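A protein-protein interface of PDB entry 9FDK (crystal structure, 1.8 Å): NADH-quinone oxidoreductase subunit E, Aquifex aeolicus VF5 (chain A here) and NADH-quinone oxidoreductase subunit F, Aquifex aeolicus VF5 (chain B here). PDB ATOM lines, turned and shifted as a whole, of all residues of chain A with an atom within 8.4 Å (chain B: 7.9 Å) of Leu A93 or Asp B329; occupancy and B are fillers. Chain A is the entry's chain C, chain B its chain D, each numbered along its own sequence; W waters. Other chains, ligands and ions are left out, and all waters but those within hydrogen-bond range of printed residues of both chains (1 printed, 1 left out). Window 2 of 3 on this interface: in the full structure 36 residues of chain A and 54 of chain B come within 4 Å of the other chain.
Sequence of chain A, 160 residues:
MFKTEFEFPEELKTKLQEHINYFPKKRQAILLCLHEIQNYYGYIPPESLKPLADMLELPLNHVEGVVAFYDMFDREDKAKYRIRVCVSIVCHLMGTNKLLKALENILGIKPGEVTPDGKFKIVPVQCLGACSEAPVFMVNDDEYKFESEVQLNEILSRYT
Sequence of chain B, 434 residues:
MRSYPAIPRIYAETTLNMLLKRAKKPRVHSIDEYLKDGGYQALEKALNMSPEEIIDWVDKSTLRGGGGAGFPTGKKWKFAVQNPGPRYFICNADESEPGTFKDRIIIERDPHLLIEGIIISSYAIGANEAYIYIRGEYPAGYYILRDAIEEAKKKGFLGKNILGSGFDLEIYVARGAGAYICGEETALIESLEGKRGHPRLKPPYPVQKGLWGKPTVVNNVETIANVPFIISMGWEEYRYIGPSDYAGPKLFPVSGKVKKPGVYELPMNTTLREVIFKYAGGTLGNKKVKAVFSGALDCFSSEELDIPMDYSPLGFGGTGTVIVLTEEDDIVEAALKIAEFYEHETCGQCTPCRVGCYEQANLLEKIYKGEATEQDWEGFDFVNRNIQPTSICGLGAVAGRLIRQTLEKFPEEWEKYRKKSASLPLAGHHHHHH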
ATOM      1  N   CYS A  86     -15.020  -4.052 -17.351  1.00  0.00           N
ATOM      2  CA  CYS A  86     -16.068  -3.629 -16.437  1.00  0.00           C
ATOM      3  C   CYS A  86     -16.430  -4.769 -15.481  1.00  0.00           C
ATOM      4  O   CYS A  86     -16.733  -5.878 -15.922  1.00  0.00           O
ATOM      5  CB  CYS A  86     -17.311  -3.165 -17.176  1.00  0.00           C
ATOM      6  SG  CYS A  86     -18.642  -2.656 -16.051  1.00  0.00           S
ATOM      7  N   VAL A  87     -16.414  -4.466 -14.179  1.00  0.00           N
ATOM      8  CA  VAL A  87     -16.715  -5.439 -13.141  1.00  0.00           C
ATOM      9  C   VAL A  87     -17.966  -5.030 -12.374  1.00  0.00           C
ATOM     10  O   VAL A  87     -18.242  -5.593 -11.315  1.00  0.00           O
ATOM     11  CB  VAL A  87     -15.512  -5.656 -12.194  1.00  0.00           C
ATOM     12  CG1 VAL A  87     -14.326  -6.265 -12.932  1.00  0.00           C
ATOM     13  CG2 VAL A  87     -15.087  -4.392 -11.435  1.00  0.00           C
ATOM     14  N   SER A  88     -18.742  -4.087 -12.917  1.00  0.00           N
ATOM     15  CA  SER A  88     -19.956  -3.583 -12.262  1.00  0.00           C
ATOM     16  C   SER A  88     -21.153  -4.494 -12.545  1.00  0.00           C
ATOM     17  O   SER A  88     -21.006  -5.506 -13.211  1.00  0.00           O
ATOM     18  CB  SER A  88     -20.239  -2.150 -12.650  1.00  0.00           C
ATOM     19  OG  SER A  88     -19.311  -1.290 -12.004  1.00  0.00           O
ATOM     20  N   ILE A  89     -22.335  -4.121 -12.039  1.00  0.00           N
ATOM     21  CA  ILE A  89     -23.460  -5.043 -11.877  1.00  0.00           C
ATOM     22  C   ILE A  89     -23.905  -5.676 -13.205  1.00  0.00           C
ATOM     23  O   ILE A  89     -24.085  -6.900 -13.266  1.00  0.00           O
ATOM     24  CB  ILE A  89     -24.630  -4.363 -11.131  1.00  0.00           C
ATOM     25  CG1 ILE A  89     -25.883  -5.247 -10.980  1.00  0.00           C
ATOM     26  CG2 ILE A  89     -25.035  -3.051 -11.781  1.00  0.00           C
ATOM     27  CD1 ILE A  89     -25.654  -6.542 -10.264  1.00  0.00           C
ATOM     28  N   VAL A  90     -24.110  -4.879 -14.266  1.00  0.00           N
ATOM     29  CA  VAL A  90     -24.713  -5.423 -15.483  1.00  0.00           C
ATOM     30  C   VAL A  90     -23.726  -6.366 -16.170  1.00  0.00           C
ATOM     31  O   VAL A  90     -24.077  -7.499 -16.514  1.00  0.00           O
ATOM     32  CB  VAL A  90     -25.248  -4.366 -16.477  1.00  0.00           C
ATOM     33  CG1 VAL A  90     -26.078  -4.992 -17.595  1.00  0.00           C
ATOM     34  CG2 VAL A  90     -26.089  -3.313 -15.774  1.00  0.00           C
ATOM     35  N   CYS A  91     -22.474  -5.936 -16.326  1.00  0.00           N
ATOM     36  CA  CYS A  91     -21.462  -6.789 -16.926  1.00  0.00           C
ATOM     37  C   CYS A  91     -21.283  -8.072 -16.120  1.00  0.00           C
ATOM     38  O   CYS A  91     -21.125  -9.146 -16.700  1.00  0.00           O
ATOM     39  CB  CYS A  91     -20.180  -6.015 -17.184  1.00  0.00           C
ATOM     40  SG  CYS A  91     -20.428  -4.723 -18.434  1.00  0.00           S
ATOM     41  N   HIS A  92     -21.337  -7.964 -14.785  1.00  0.00           N
ATOM     42  CA  HIS A  92     -21.162  -9.137 -13.954  1.00  0.00           C
ATOM     43  C   HIS A  92     -22.278 -10.134 -14.250  1.00  0.00           C
ATOM     44  O   HIS A  92     -22.013 -11.311 -14.483  1.00  0.00           O
ATOM     45  CB  HIS A  92     -21.072  -8.753 -12.474  1.00  0.00           C
ATOM     46  CG  HIS A  92     -21.029  -9.964 -11.613  1.00  0.00           C
ATOM     47  ND1 HIS A  92     -19.899 -10.740 -11.434  1.00  0.00           N
ATOM     48  CD2 HIS A  92     -22.030 -10.572 -10.961  1.00  0.00           C
ATOM     49  CE1 HIS A  92     -20.210 -11.767 -10.651  1.00  0.00           C
ATOM     50  NE2 HIS A  92     -21.499 -11.694 -10.363  1.00  0.00           N
ATOM     51  N   LEU A  93     -23.516  -9.631 -14.261  1.00  0.00           N
ATOM     52  CA  LEU A  93     -24.708 -10.409 -14.563  1.00  0.00           C
ATOM     53  C   LEU A  93     -24.606 -11.086 -15.932  1.00  0.00           C
ATOM     54  O   LEU A  93     -25.005 -12.230 -16.091  1.00  0.00           O
ATOM     55  CB  LEU A  93     -25.869  -9.424 -14.525  1.00  0.00           C
ATOM     56  CG  LEU A  93     -27.248  -9.994 -14.202  1.00  0.00           C
ATOM     57  CD1 LEU A  93     -27.293 -10.573 -12.787  1.00  0.00           C
ATOM     58  CD2 LEU A  93     -28.255  -8.867 -14.384  1.00  0.00           C
ATOM     59  N   MET A  94     -24.034 -10.393 -16.920  1.00  0.00           N
ATOM     60  CA  MET A  94     -24.082 -10.872 -18.292  1.00  0.00           C
ATOM     61  C   MET A  94     -22.795 -11.569 -18.746  1.00  0.00           C
ATOM     62  O   MET A  94     -22.772 -12.051 -19.874  1.00  0.00           O
ATOM     63  CB  MET A  94     -24.415  -9.725 -19.248  1.00  0.00           C
ATOM     64  CG  MET A  94     -25.678  -8.983 -18.881  1.00  0.00           C
ATOM     65  SD  MET A  94     -27.155 -10.008 -18.825  1.00  0.00           S
ATOM     66  CE  MET A  94     -27.344 -10.578 -20.521  1.00  0.00           C
ATOM     67  N   GLY A  95     -21.732 -11.599 -17.924  1.00  0.00           N
ATOM     68  CA  GLY A  95     -20.616 -12.525 -18.123  1.00  0.00           C
ATOM     69  C   GLY A  95     -19.198 -11.944 -17.996  1.00  0.00           C
ATOM     70  O   GLY A  95     -18.284 -12.442 -18.669  1.00  0.00           O
ATOM     71  N   THR A  96     -18.968 -10.962 -17.102  1.00  0.00           N
ATOM     72  CA  THR A  96     -17.612 -10.496 -16.814  1.00  0.00           C
ATOM     73  C   THR A  96     -16.668 -11.682 -16.604  1.00  0.00           C
ATOM     74  O   THR A  96     -15.539 -11.654 -17.077  1.00  0.00           O
ATOM     75  CB  THR A  96     -17.584  -9.586 -15.584  1.00  0.00           C
ATOM     76  OG1 THR A  96     -18.318  -8.417 -15.917  1.00  0.00           O
ATOM     77  CG2 THR A  96     -16.189  -9.142 -15.180  1.00  0.00           C
ATOM     78  N   ASN A  97     -17.104 -12.708 -15.863  1.00  0.00           N
ATOM     79  CA  ASN A  97     -16.217 -13.796 -15.485  1.00  0.00           C
ATOM     80  C   ASN A  97     -15.762 -14.608 -16.698  1.00  0.00           C
ATOM     81  O   ASN A  97     -14.647 -15.107 -16.692  1.00  0.00           O
ATOM     82  CB  ASN A  97     -16.826 -14.682 -14.405  1.00  0.00           C
ATOM     83  CG  ASN A  97     -16.839 -14.012 -13.047  1.00  0.00           C
ATOM     84  OD1 ASN A  97     -16.203 -12.966 -12.839  1.00  0.00           O
ATOM     85  ND2 ASN A  97     -17.589 -14.578 -12.116  1.00  0.00           N
ATOM     86  N   LYS A  98     -16.606 -14.737 -17.727  1.00  0.00           N
ATOM     87  CA  LYS A  98     -16.229 -15.422 -18.959  1.00  0.00           C
ATOM     88  C   LYS A  98     -15.185 -14.622 -19.738  1.00  0.00           C
ATOM     89  O   LYS A  98     -14.262 -15.192 -20.307  1.00  0.00           O
ATOM     90  CB  LYS A  98     -17.447 -15.635 -19.862  1.00  0.00           C
ATOM     91  CG  LYS A  98     -18.498 -16.538 -19.266  1.00  0.00           C
ATOM     92  CD  LYS A  98     -19.775 -16.625 -20.092  1.00  0.00           C
ATOM     93  CE  LYS A  98     -20.785 -17.553 -19.475  1.00  0.00           C
ATOM     94  NZ  LYS A  98     -22.068 -17.494 -20.188  1.00  0.00           N
ATOM     95  N   ALA A 134     -23.264  -5.466 -22.545  1.00  0.00           N
ATOM     96  CA  ALA A 134     -22.502  -6.187 -21.533  1.00  0.00           C
ATOM     97  C   ALA A 134     -22.177  -7.597 -22.012  1.00  0.00           C
ATOM     98  O   ALA A 134     -22.968  -8.196 -22.746  1.00  0.00           O
ATOM     99  CB  ALA A 134     -23.304  -6.245 -20.246  1.00  0.00           C
ATOM    100  N   PRO A 135     -21.023  -8.194 -21.638  1.00  0.00           N
ATOM    101  CA  PRO A 135     -19.970  -7.540 -20.858  1.00  0.00           C
ATOM    102  C   PRO A 135     -18.998  -6.720 -21.705  1.00  0.00           C
ATOM    103  O   PRO A 135     -18.590  -7.161 -22.775  1.00  0.00           O
ATOM    104  CB  PRO A 135     -19.271  -8.718 -20.189  1.00  0.00           C
ATOM    105  CG  PRO A 135     -19.525  -9.916 -21.070  1.00  0.00           C
ATOM    106  CD  PRO A 135     -20.705  -9.594 -21.953  1.00  0.00           C
ATOM    107  N   SER B 255     -31.214  -2.448 -19.695  1.00  0.00           N
ATOM    108  CA  SER B 255     -30.168  -3.445 -19.769  1.00  0.00           C
ATOM    109  C   SER B 255     -30.488  -4.639 -18.864  1.00  0.00           C
ATOM    110  O   SER B 255     -31.526  -4.692 -18.201  1.00  0.00           O
ATOM    111  CB  SER B 255     -28.827  -2.821 -19.443  1.00  0.00           C
ATOM    112  OG  SER B 255     -28.748  -2.389 -18.090  1.00  0.00           O
ATOM    113  N   GLY B 256     -29.601  -5.626 -18.911  1.00  0.00           N
ATOM    114  CA  GLY B 256     -29.775  -6.855 -18.169  1.00  0.00           C
ATOM    115  C   GLY B 256     -30.583  -7.840 -19.000  1.00  0.00           C
ATOM    116  O   GLY B 256     -30.406  -7.919 -20.216  1.00  0.00           O
ATOM    117  N   LYS B 257     -31.535  -8.504 -18.350  1.00  0.00           N
ATOM    118  CA  LYS B 257     -32.129  -9.718 -18.875  1.00  0.00           C
ATOM    119  C   LYS B 257     -33.359  -9.403 -19.725  1.00  0.00           C
ATOM    120  O   LYS B 257     -34.416  -9.996 -19.534  1.00  0.00           O
ATOM    121  CB  LYS B 257     -32.490 -10.658 -17.725  1.00  0.00           C
ATOM    122  CG  LYS B 257     -31.332 -11.110 -16.855  1.00  0.00           C
ATOM    123  CD  LYS B 257     -30.353 -11.998 -17.609  1.00  0.00           C
ATOM    124  CE  LYS B 257     -29.208 -12.423 -16.743  1.00  0.00           C
ATOM    125  NZ  LYS B 257     -29.625 -13.432 -15.767  1.00  0.00           N
ATOM    126  N   LYS B 287     -38.164 -15.621 -18.886  1.00  0.00           N
ATOM    127  CA  LYS B 287     -38.171 -15.846 -17.448  1.00  0.00           C
ATOM    128  C   LYS B 287     -38.913 -14.711 -16.741  1.00  0.00           C
ATOM    129  O   LYS B 287     -39.025 -13.598 -17.252  1.00  0.00           O
ATOM    130  CB  LYS B 287     -36.732 -15.961 -16.938  1.00  0.00           C
ATOM    131  CG  LYS B 287     -35.877 -17.038 -17.606  1.00  0.00           C
ATOM    132  CD  LYS B 287     -34.488 -17.098 -16.977  1.00  0.00           C
ATOM    133  CE  LYS B 287     -33.531 -18.047 -17.627  1.00  0.00           C
ATOM    134  NZ  LYS B 287     -34.097 -19.396 -17.593  1.00  0.00           N
ATOM    135  N   LYS B 288     -39.381 -14.990 -15.526  1.00  0.00           N
ATOM    136  CA  LYS B 288     -40.103 -13.992 -14.752  1.00  0.00           C
ATOM    137  C   LYS B 288     -39.145 -12.899 -14.294  1.00  0.00           C
ATOM    138  O   LYS B 288     -37.984 -13.155 -13.983  1.00  0.00           O
ATOM    139  CB  LYS B 288     -40.813 -14.659 -13.571  1.00  0.00           C
ATOM    140  CG  LYS B 288     -41.961 -15.553 -14.034  1.00  0.00           C
ATOM    141  CD  LYS B 288     -42.620 -16.327 -12.912  1.00  0.00           C
ATOM    142  CE  LYS B 288     -43.630 -17.283 -13.476  1.00  0.00           C
ATOM    143  NZ  LYS B 288     -44.079 -18.199 -12.424  1.00  0.00           N
ATOM    144  N   LYS B 290     -37.638 -10.662 -11.614  1.00  0.00           N
ATOM    145  CA  LYS B 290     -37.472 -10.734 -10.167  1.00  0.00           C
ATOM    146  C   LYS B 290     -37.354  -9.325  -9.583  1.00  0.00           C
ATOM    147  O   LYS B 290     -37.990  -9.010  -8.582  1.00  0.00           O
ATOM    148  CB  LYS B 290     -36.215 -11.521  -9.778  1.00  0.00           C
ATOM    149  CG  LYS B 290     -35.946 -11.512  -8.272  1.00  0.00           C
ATOM    150  CD  LYS B 290     -34.672 -12.217  -7.817  1.00  0.00           C
ATOM    151  CE  LYS B 290     -34.847 -13.693  -7.763  1.00  0.00           C
ATOM    152  NZ  LYS B 290     -33.621 -14.358  -7.318  1.00  0.00           N
ATOM    153  N   ALA B 291     -36.518  -8.482 -10.200  1.00  0.00           N
ATOM    154  CA  ALA B 291     -36.333  -7.121  -9.729  1.00  0.00           C
ATOM    155  C   ALA B 291     -35.877  -6.230 -10.877  1.00  0.00           C
ATOM    156  O   ALA B 291     -35.327  -6.719 -11.863  1.00  0.00           O
ATOM    157  CB  ALA B 291     -35.320  -7.086  -8.601  1.00  0.00           C
ATOM    158  N   PHE B 293     -33.414  -2.838 -10.999  1.00  0.00           N
ATOM    159  CA  PHE B 293     -32.583  -1.829 -10.347  1.00  0.00           C
ATOM    160  C   PHE B 293     -32.635  -0.549 -11.177  1.00  0.00           C
ATOM    161  O   PHE B 293     -32.403  -0.598 -12.385  1.00  0.00           O
ATOM    162  CB  PHE B 293     -31.134  -2.296 -10.218  1.00  0.00           C
ATOM    163  CG  PHE B 293     -30.856  -3.392  -9.206  1.00  0.00           C
ATOM    164  CD1 PHE B 293     -31.887  -4.020  -8.514  1.00  0.00           C
ATOM    165  CD2 PHE B 293     -29.551  -3.827  -8.993  1.00  0.00           C
ATOM    166  CE1 PHE B 293     -31.613  -5.033  -7.606  1.00  0.00           C
ATOM    167  CE2 PHE B 293     -29.277  -4.829  -8.074  1.00  0.00           C
ATOM    168  CZ  PHE B 293     -30.311  -5.424  -7.381  1.00  0.00           C
ATOM    169  N   ILE B 323     -32.396  -1.715 -15.126  1.00  0.00           N
ATOM    170  CA  ILE B 323     -31.619  -2.942 -15.171  1.00  0.00           C
ATOM    171  C   ILE B 323     -32.531  -4.083 -14.724  1.00  0.00           C
ATOM    172  O   ILE B 323     -32.966  -4.082 -13.578  1.00  0.00           O
ATOM    173  CB  ILE B 323     -30.388  -2.854 -14.249  1.00  0.00           C
ATOM    174  CG1 ILE B 323     -29.486  -1.653 -14.545  1.00  0.00           C
ATOM    175  CG2 ILE B 323     -29.632  -4.181 -14.306  1.00  0.00           C
ATOM    176  CD1 ILE B 323     -28.499  -1.326 -13.429  1.00  0.00           C
ATOM    177  N   VAL B 324     -32.747  -5.099 -15.582  1.00  0.00           N
ATOM    178  CA  VAL B 324     -33.714  -6.150 -15.308  1.00  0.00           C
ATOM    179  C   VAL B 324     -32.983  -7.410 -14.835  1.00  0.00           C
ATOM    180  O   VAL B 324     -32.087  -7.911 -15.515  1.00  0.00           O
ATOM    181  CB  VAL B 324     -34.589  -6.428 -16.551  1.00  0.00           C
ATOM    182  CG1 VAL B 324     -35.592  -7.551 -16.307  1.00  0.00           C
ATOM    183  CG2 VAL B 324     -35.323  -5.191 -17.044  1.00  0.00           C
ATOM    184  N   LEU B 325     -33.376  -7.912 -13.656  1.00  0.00           N
ATOM    185  CA  LEU B 325     -32.956  -9.206 -13.135  1.00  0.00           C
ATOM    186  C   LEU B 325     -34.144 -10.166 -13.196  1.00  0.00           C
ATOM    187  O   LEU B 325     -35.270  -9.789 -12.858  1.00  0.00           O
ATOM    188  CB  LEU B 325     -32.482  -9.033 -11.693  1.00  0.00           C
ATOM    189  CG  LEU B 325     -31.166  -8.271 -11.463  1.00  0.00           C
ATOM    190  CD1 LEU B 325     -31.377  -6.802 -11.561  1.00  0.00           C
ATOM    191  CD2 LEU B 325     -30.623  -8.613 -10.077  1.00  0.00           C
ATOM    192  N   THR B 326     -33.892 -11.420 -13.574  1.00  0.00           N
ATOM    193  CA  THR B 326     -34.951 -12.418 -13.628  1.00  0.00           C
ATOM    194  C   THR B 326     -34.794 -13.437 -12.503  1.00  0.00           C
ATOM    195  O   THR B 326     -33.936 -13.307 -11.634  1.00  0.00           O
ATOM    196  CB  THR B 326     -35.005 -13.076 -15.010  1.00  0.00           C
ATOM    197  OG1 THR B 326     -33.684 -13.493 -15.354  1.00  0.00           O
ATOM    198  CG2 THR B 326     -35.542 -12.101 -16.035  1.00  0.00           C
ATOM    199  N   GLU B 327     -35.672 -14.433 -12.530  1.00  0.00           N
ATOM    200  CA  GLU B 327     -35.961 -15.294 -11.390  1.00  0.00           C
ATOM    201  C   GLU B 327     -34.735 -16.052 -10.885  1.00  0.00           C
ATOM    202  O   GLU B 327     -34.679 -16.385  -9.704  1.00  0.00           O
ATOM    203  CB  GLU B 327     -37.073 -16.270 -11.755  1.00  0.00           C
ATOM    204  CG  GLU B 327     -36.833 -17.051 -13.042  1.00  0.00           C
ATOM    205  CD  GLU B 327     -38.049 -17.892 -13.395  1.00  0.00           C
ATOM    206  OE1 GLU B 327     -38.283 -18.885 -12.669  1.00  0.00           O
ATOM    207  OE2 GLU B 327     -38.779 -17.563 -14.358  1.00  0.00           O
ATOM    208  N   GLU B 328     -33.750 -16.319 -11.751  1.00  0.00           N
ATOM    209  CA  GLU B 328     -32.606 -17.100 -11.312  1.00  0.00           C
ATOM    210  C   GLU B 328     -31.469 -16.223 -10.804  1.00  0.00           C
ATOM    211  O   GLU B 328     -30.490 -16.760 -10.300  1.00  0.00           O
ATOM    212  CB  GLU B 328     -32.092 -18.021 -12.414  1.00  0.00           C
ATOM    213  CG  GLU B 328     -33.032 -19.198 -12.643  1.00  0.00           C
ATOM    214  CD  GLU B 328     -32.331 -20.318 -13.380  1.00  0.00           C
ATOM    215  OE1 GLU B 328     -31.510 -20.986 -12.716  1.00  0.00           O
ATOM    216  OE2 GLU B 328     -32.589 -20.503 -14.586  1.00  0.00           O
ATOM    217  N   ASP B 329     -31.605 -14.895 -10.895  1.00  0.00           N
ATOM    218  CA  ASP B 329     -30.531 -14.001 -10.487  1.00  0.00           C
ATOM    219  C   ASP B 329     -30.502 -13.846  -8.969  1.00  0.00           C
ATOM    220  O   ASP B 329     -31.515 -13.541  -8.356  1.00  0.00           O
ATOM    221  CB  ASP B 329     -30.621 -12.677 -11.219  1.00  0.00           C
ATOM    222  CG  ASP B 329     -30.410 -12.825 -12.720  1.00  0.00           C
ATOM    223  OD1 ASP B 329     -29.571 -13.678 -13.098  1.00  0.00           O
ATOM    224  OD2 ASP B 329     -31.091 -12.123 -13.493  1.00  0.00           O
ATOM    225  N   ASP B 330     -29.310 -14.032  -8.389  1.00  0.00           N
ATOM    226  CA  ASP B 330     -29.112 -13.974  -6.948  1.00  0.00           C
ATOM    227  C   ASP B 330     -29.102 -12.502  -6.517  1.00  0.00           C
ATOM    228  O   ASP B 330     -28.248 -11.729  -6.948  1.00  0.00           O
ATOM    229  CB  ASP B 330     -27.868 -14.775  -6.580  1.00  0.00           C
ATOM    230  CG  ASP B 330     -27.492 -14.818  -5.103  1.00  0.00           C
ATOM    231  OD1 ASP B 330     -27.730 -13.830  -4.388  1.00  0.00           O
ATOM    232  OD2 ASP B 330     -26.919 -15.830  -4.691  1.00  0.00           O
ATOM    233  N   ILE B 331     -30.077 -12.104  -5.686  1.00  0.00           N
ATOM    234  CA  ILE B 331     -30.226 -10.714  -5.275  1.00  0.00           C
ATOM    235  C   ILE B 331     -29.043 -10.276  -4.409  1.00  0.00           C
ATOM    236  O   ILE B 331     -28.673  -9.105  -4.434  1.00  0.00           O
ATOM    237  CB  ILE B 331     -31.561 -10.475  -4.542  1.00  0.00           C
ATOM    238  CG1 ILE B 331     -31.993  -9.021  -4.635  1.00  0.00           C
ATOM    239  CG2 ILE B 331     -31.496 -10.943  -3.091  1.00  0.00           C
ATOM    240  CD1 ILE B 331     -32.586  -8.649  -5.989  1.00  0.00           C
ATOM    241  N   VAL B 332     -28.474 -11.198  -3.624  1.00  0.00           N
ATOM    242  CA  VAL B 332     -27.386 -10.845  -2.728  1.00  0.00           C
ATOM    243  C   VAL B 332     -26.107 -10.608  -3.544  1.00  0.00           C
ATOM    244  O   VAL B 332     -25.341  -9.690  -3.266  1.00  0.00           O
ATOM    245  CB  VAL B 332     -27.191 -11.920  -1.646  1.00  0.00           C
ATOM    246  CG1 VAL B 332     -26.006 -11.595  -0.742  1.00  0.00           C
ATOM    247  CG2 VAL B 332     -28.461 -12.104  -0.816  1.00  0.00           C
ATOM    248  N   GLU B 333     -25.888 -11.433  -4.565  1.00  0.00           N
ATOM    249  CA  GLU B 333     -24.769 -11.232  -5.470  1.00  0.00           C
ATOM    250  C   GLU B 333     -24.888  -9.862  -6.133  1.00  0.00           C
ATOM    251  O   GLU B 333     -23.898  -9.124  -6.250  1.00  0.00           O
ATOM    252  CB  GLU B 333     -24.765 -12.405  -6.443  1.00  0.00           C
ATOM    253  CG  GLU B 333     -23.647 -12.362  -7.474  1.00  0.00           C
ATOM    254  CD  GLU B 333     -23.755 -13.509  -8.466  1.00  0.00           C
ATOM    255  OE1 GLU B 333     -24.652 -14.378  -8.375  1.00  0.00           O
ATOM    256  OE2 GLU B 333     -22.903 -13.496  -9.352  1.00  0.00           O
ATOM    257  N   ALA B 334     -26.118  -9.508  -6.547  1.00  0.00           N
ATOM    258  CA  ALA B 334     -26.352  -8.228  -7.198  1.00  0.00           C
ATOM    259  C   ALA B 334     -26.096  -7.080  -6.225  1.00  0.00           C
ATOM    260  O   ALA B 334     -25.455  -6.079  -6.577  1.00  0.00           O
ATOM    261  CB  ALA B 334     -27.764  -8.179  -7.764  1.00  0.00           C
ATOM    262  N   LYS B 337     -22.473  -6.248  -5.861  1.00  0.00           N
ATOM    263  CA  LYS B 337     -21.944  -5.411  -6.925  1.00  0.00           C
ATOM    264  C   LYS B 337     -22.277  -3.941  -6.670  1.00  0.00           C
ATOM    265  O   LYS B 337     -21.477  -3.066  -6.991  1.00  0.00           O
ATOM    266  CB  LYS B 337     -22.401  -5.926  -8.296  1.00  0.00           C
ATOM    267  CG  LYS B 337     -21.749  -7.241  -8.699  1.00  0.00           C
ATOM    268  CD  LYS B 337     -20.321  -6.998  -9.184  1.00  0.00           C
ATOM    269  CE  LYS B 337     -19.449  -8.209  -9.151  1.00  0.00           C
ATOM    270  NZ  LYS B 337     -18.921  -8.512  -7.828  1.00  0.00           N
ATOM    271  N   PHE B 410     -36.700  -8.790  -0.464  1.00  0.00           N
ATOM    272  CA  PHE B 410     -36.286 -10.163  -0.724  1.00  0.00           C
ATOM    273  C   PHE B 410     -35.703 -10.805   0.530  1.00  0.00           C
ATOM    274  O   PHE B 410     -34.591 -11.325   0.488  1.00  0.00           O
ATOM    275  CB  PHE B 410     -35.271 -10.198  -1.869  1.00  0.00           C
ATOM    276  CG  PHE B 410     -35.867  -9.652  -3.155  1.00  0.00           C
ATOM    277  CD1 PHE B 410     -36.622 -10.469  -3.984  1.00  0.00           C
ATOM    278  CD2 PHE B 410     -35.718  -8.318  -3.487  1.00  0.00           C
ATOM    279  CE1 PHE B 410     -37.178  -9.961  -5.145  1.00  0.00           C
ATOM    280  CE2 PHE B 410     -36.278  -7.808  -4.645  1.00  0.00           C
ATOM    281  CZ  PHE B 410     -37.006  -8.627  -5.469  1.00  0.00           C
ATOM    282  N   GLU B 413     -34.202 -14.569   0.361  1.00  0.00           N
ATOM    283  CA  GLU B 413     -32.888 -14.804  -0.225  1.00  0.00           C
ATOM    284  C   GLU B 413     -31.766 -14.461   0.756  1.00  0.00           C
ATOM    285  O   GLU B 413     -30.777 -15.189   0.841  1.00  0.00           O
ATOM    286  CB  GLU B 413     -32.673 -14.033  -1.525  1.00  0.00           C
ATOM    287  CG  GLU B 413     -33.320 -14.756  -2.701  1.00  0.00           C
ATOM    288  CD  GLU B 413     -33.083 -14.078  -4.035  1.00  0.00           C
ATOM    289  OE1 GLU B 413     -34.092 -13.677  -4.644  1.00  0.00           O
ATOM    290  OE2 GLU B 413     -31.916 -14.000  -4.467  1.00  0.00           O
HETATM  291  O   HOH W   1     -21.906  -2.297  -9.791  1.00  0.00           O
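Printed residues of chain B that touch a printed residue of chain A: Ser B255, Gly B256, Lys B257, Ile B323, Asp B329, Glu B333, Ala B334 and Lys B337. Hydrophobic or aromatic side chains of chain B that line the printed part of chain A: Ile B323 and Ala B334. Among the printed residues, 10 pairs touch across the chains.
Leu A93 touches one residue of chain B. Ala A134 touches none of the printed residues of chain B. Of the printed residues of chain A, Ser B255 touches Val A90. Printed residues of chain A within 4 Å of Lys B257: Met A94. Of the printed residues of chain A, Glu B333 touches His A92 (2.5 Å). Printed residues of chain A within 4 Å of Lys B337: Val A87, Ile A89 and His A92. The nearest residue of chain B that does not touch Leu A93 is Lys B257 (4.02 Å). The nearest residue of chain A that does not touch Asp B329 is Met A94 (7.0 Å). The nearest printed residue of chain B that does not touch Met A94 is Gly B256 (4.1 Å).
Among the printed residues, pairs that only touch across the chains: Val A87 with Lys B337, His A92 with Lys B337, Ile A89 with Ala B334, Val A90 with Ser B255, Met A94 with Lys B257, Val A90 with Gly B256, Ile A89 with Lys B337, Leu A93 with Asp B329 and Val A90 with Ile B323.
Water W1 lies within hydrogen-bond range of N of Ile A89 and O of Lys B337.
NZ of Lys B290 lies within hydrogen-bond range of O of Asp B329, at 2.5 Å. The backbone NH (N) of Phe B293 is in hydrogen-bond range of the backbone carbonyl oxygen (O) of Ile B323 (2.9 Å). The backbone NH (N) of Lys B257 lies within hydrogen-bond range of the backbone carbonyl oxygen (O) of Val B324 (2.9 Å). N of Glu B333 sits at hydrogen-bond distance from OD1 of Asp B330 (3.0 Å). N of Thr B326 sits at hydrogen-bond distance from OD2 of Asp B329. The side-chain amino group (NZ) of Lys B257 is in salt-bridge range of the side-chain carboxylate (OD1) of Asp B329.
A ring nitrogen (NE2) of His A92 lies within hydrogen-bond range of the side-chain carboxylate of Glu B333 (2.5 Å).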
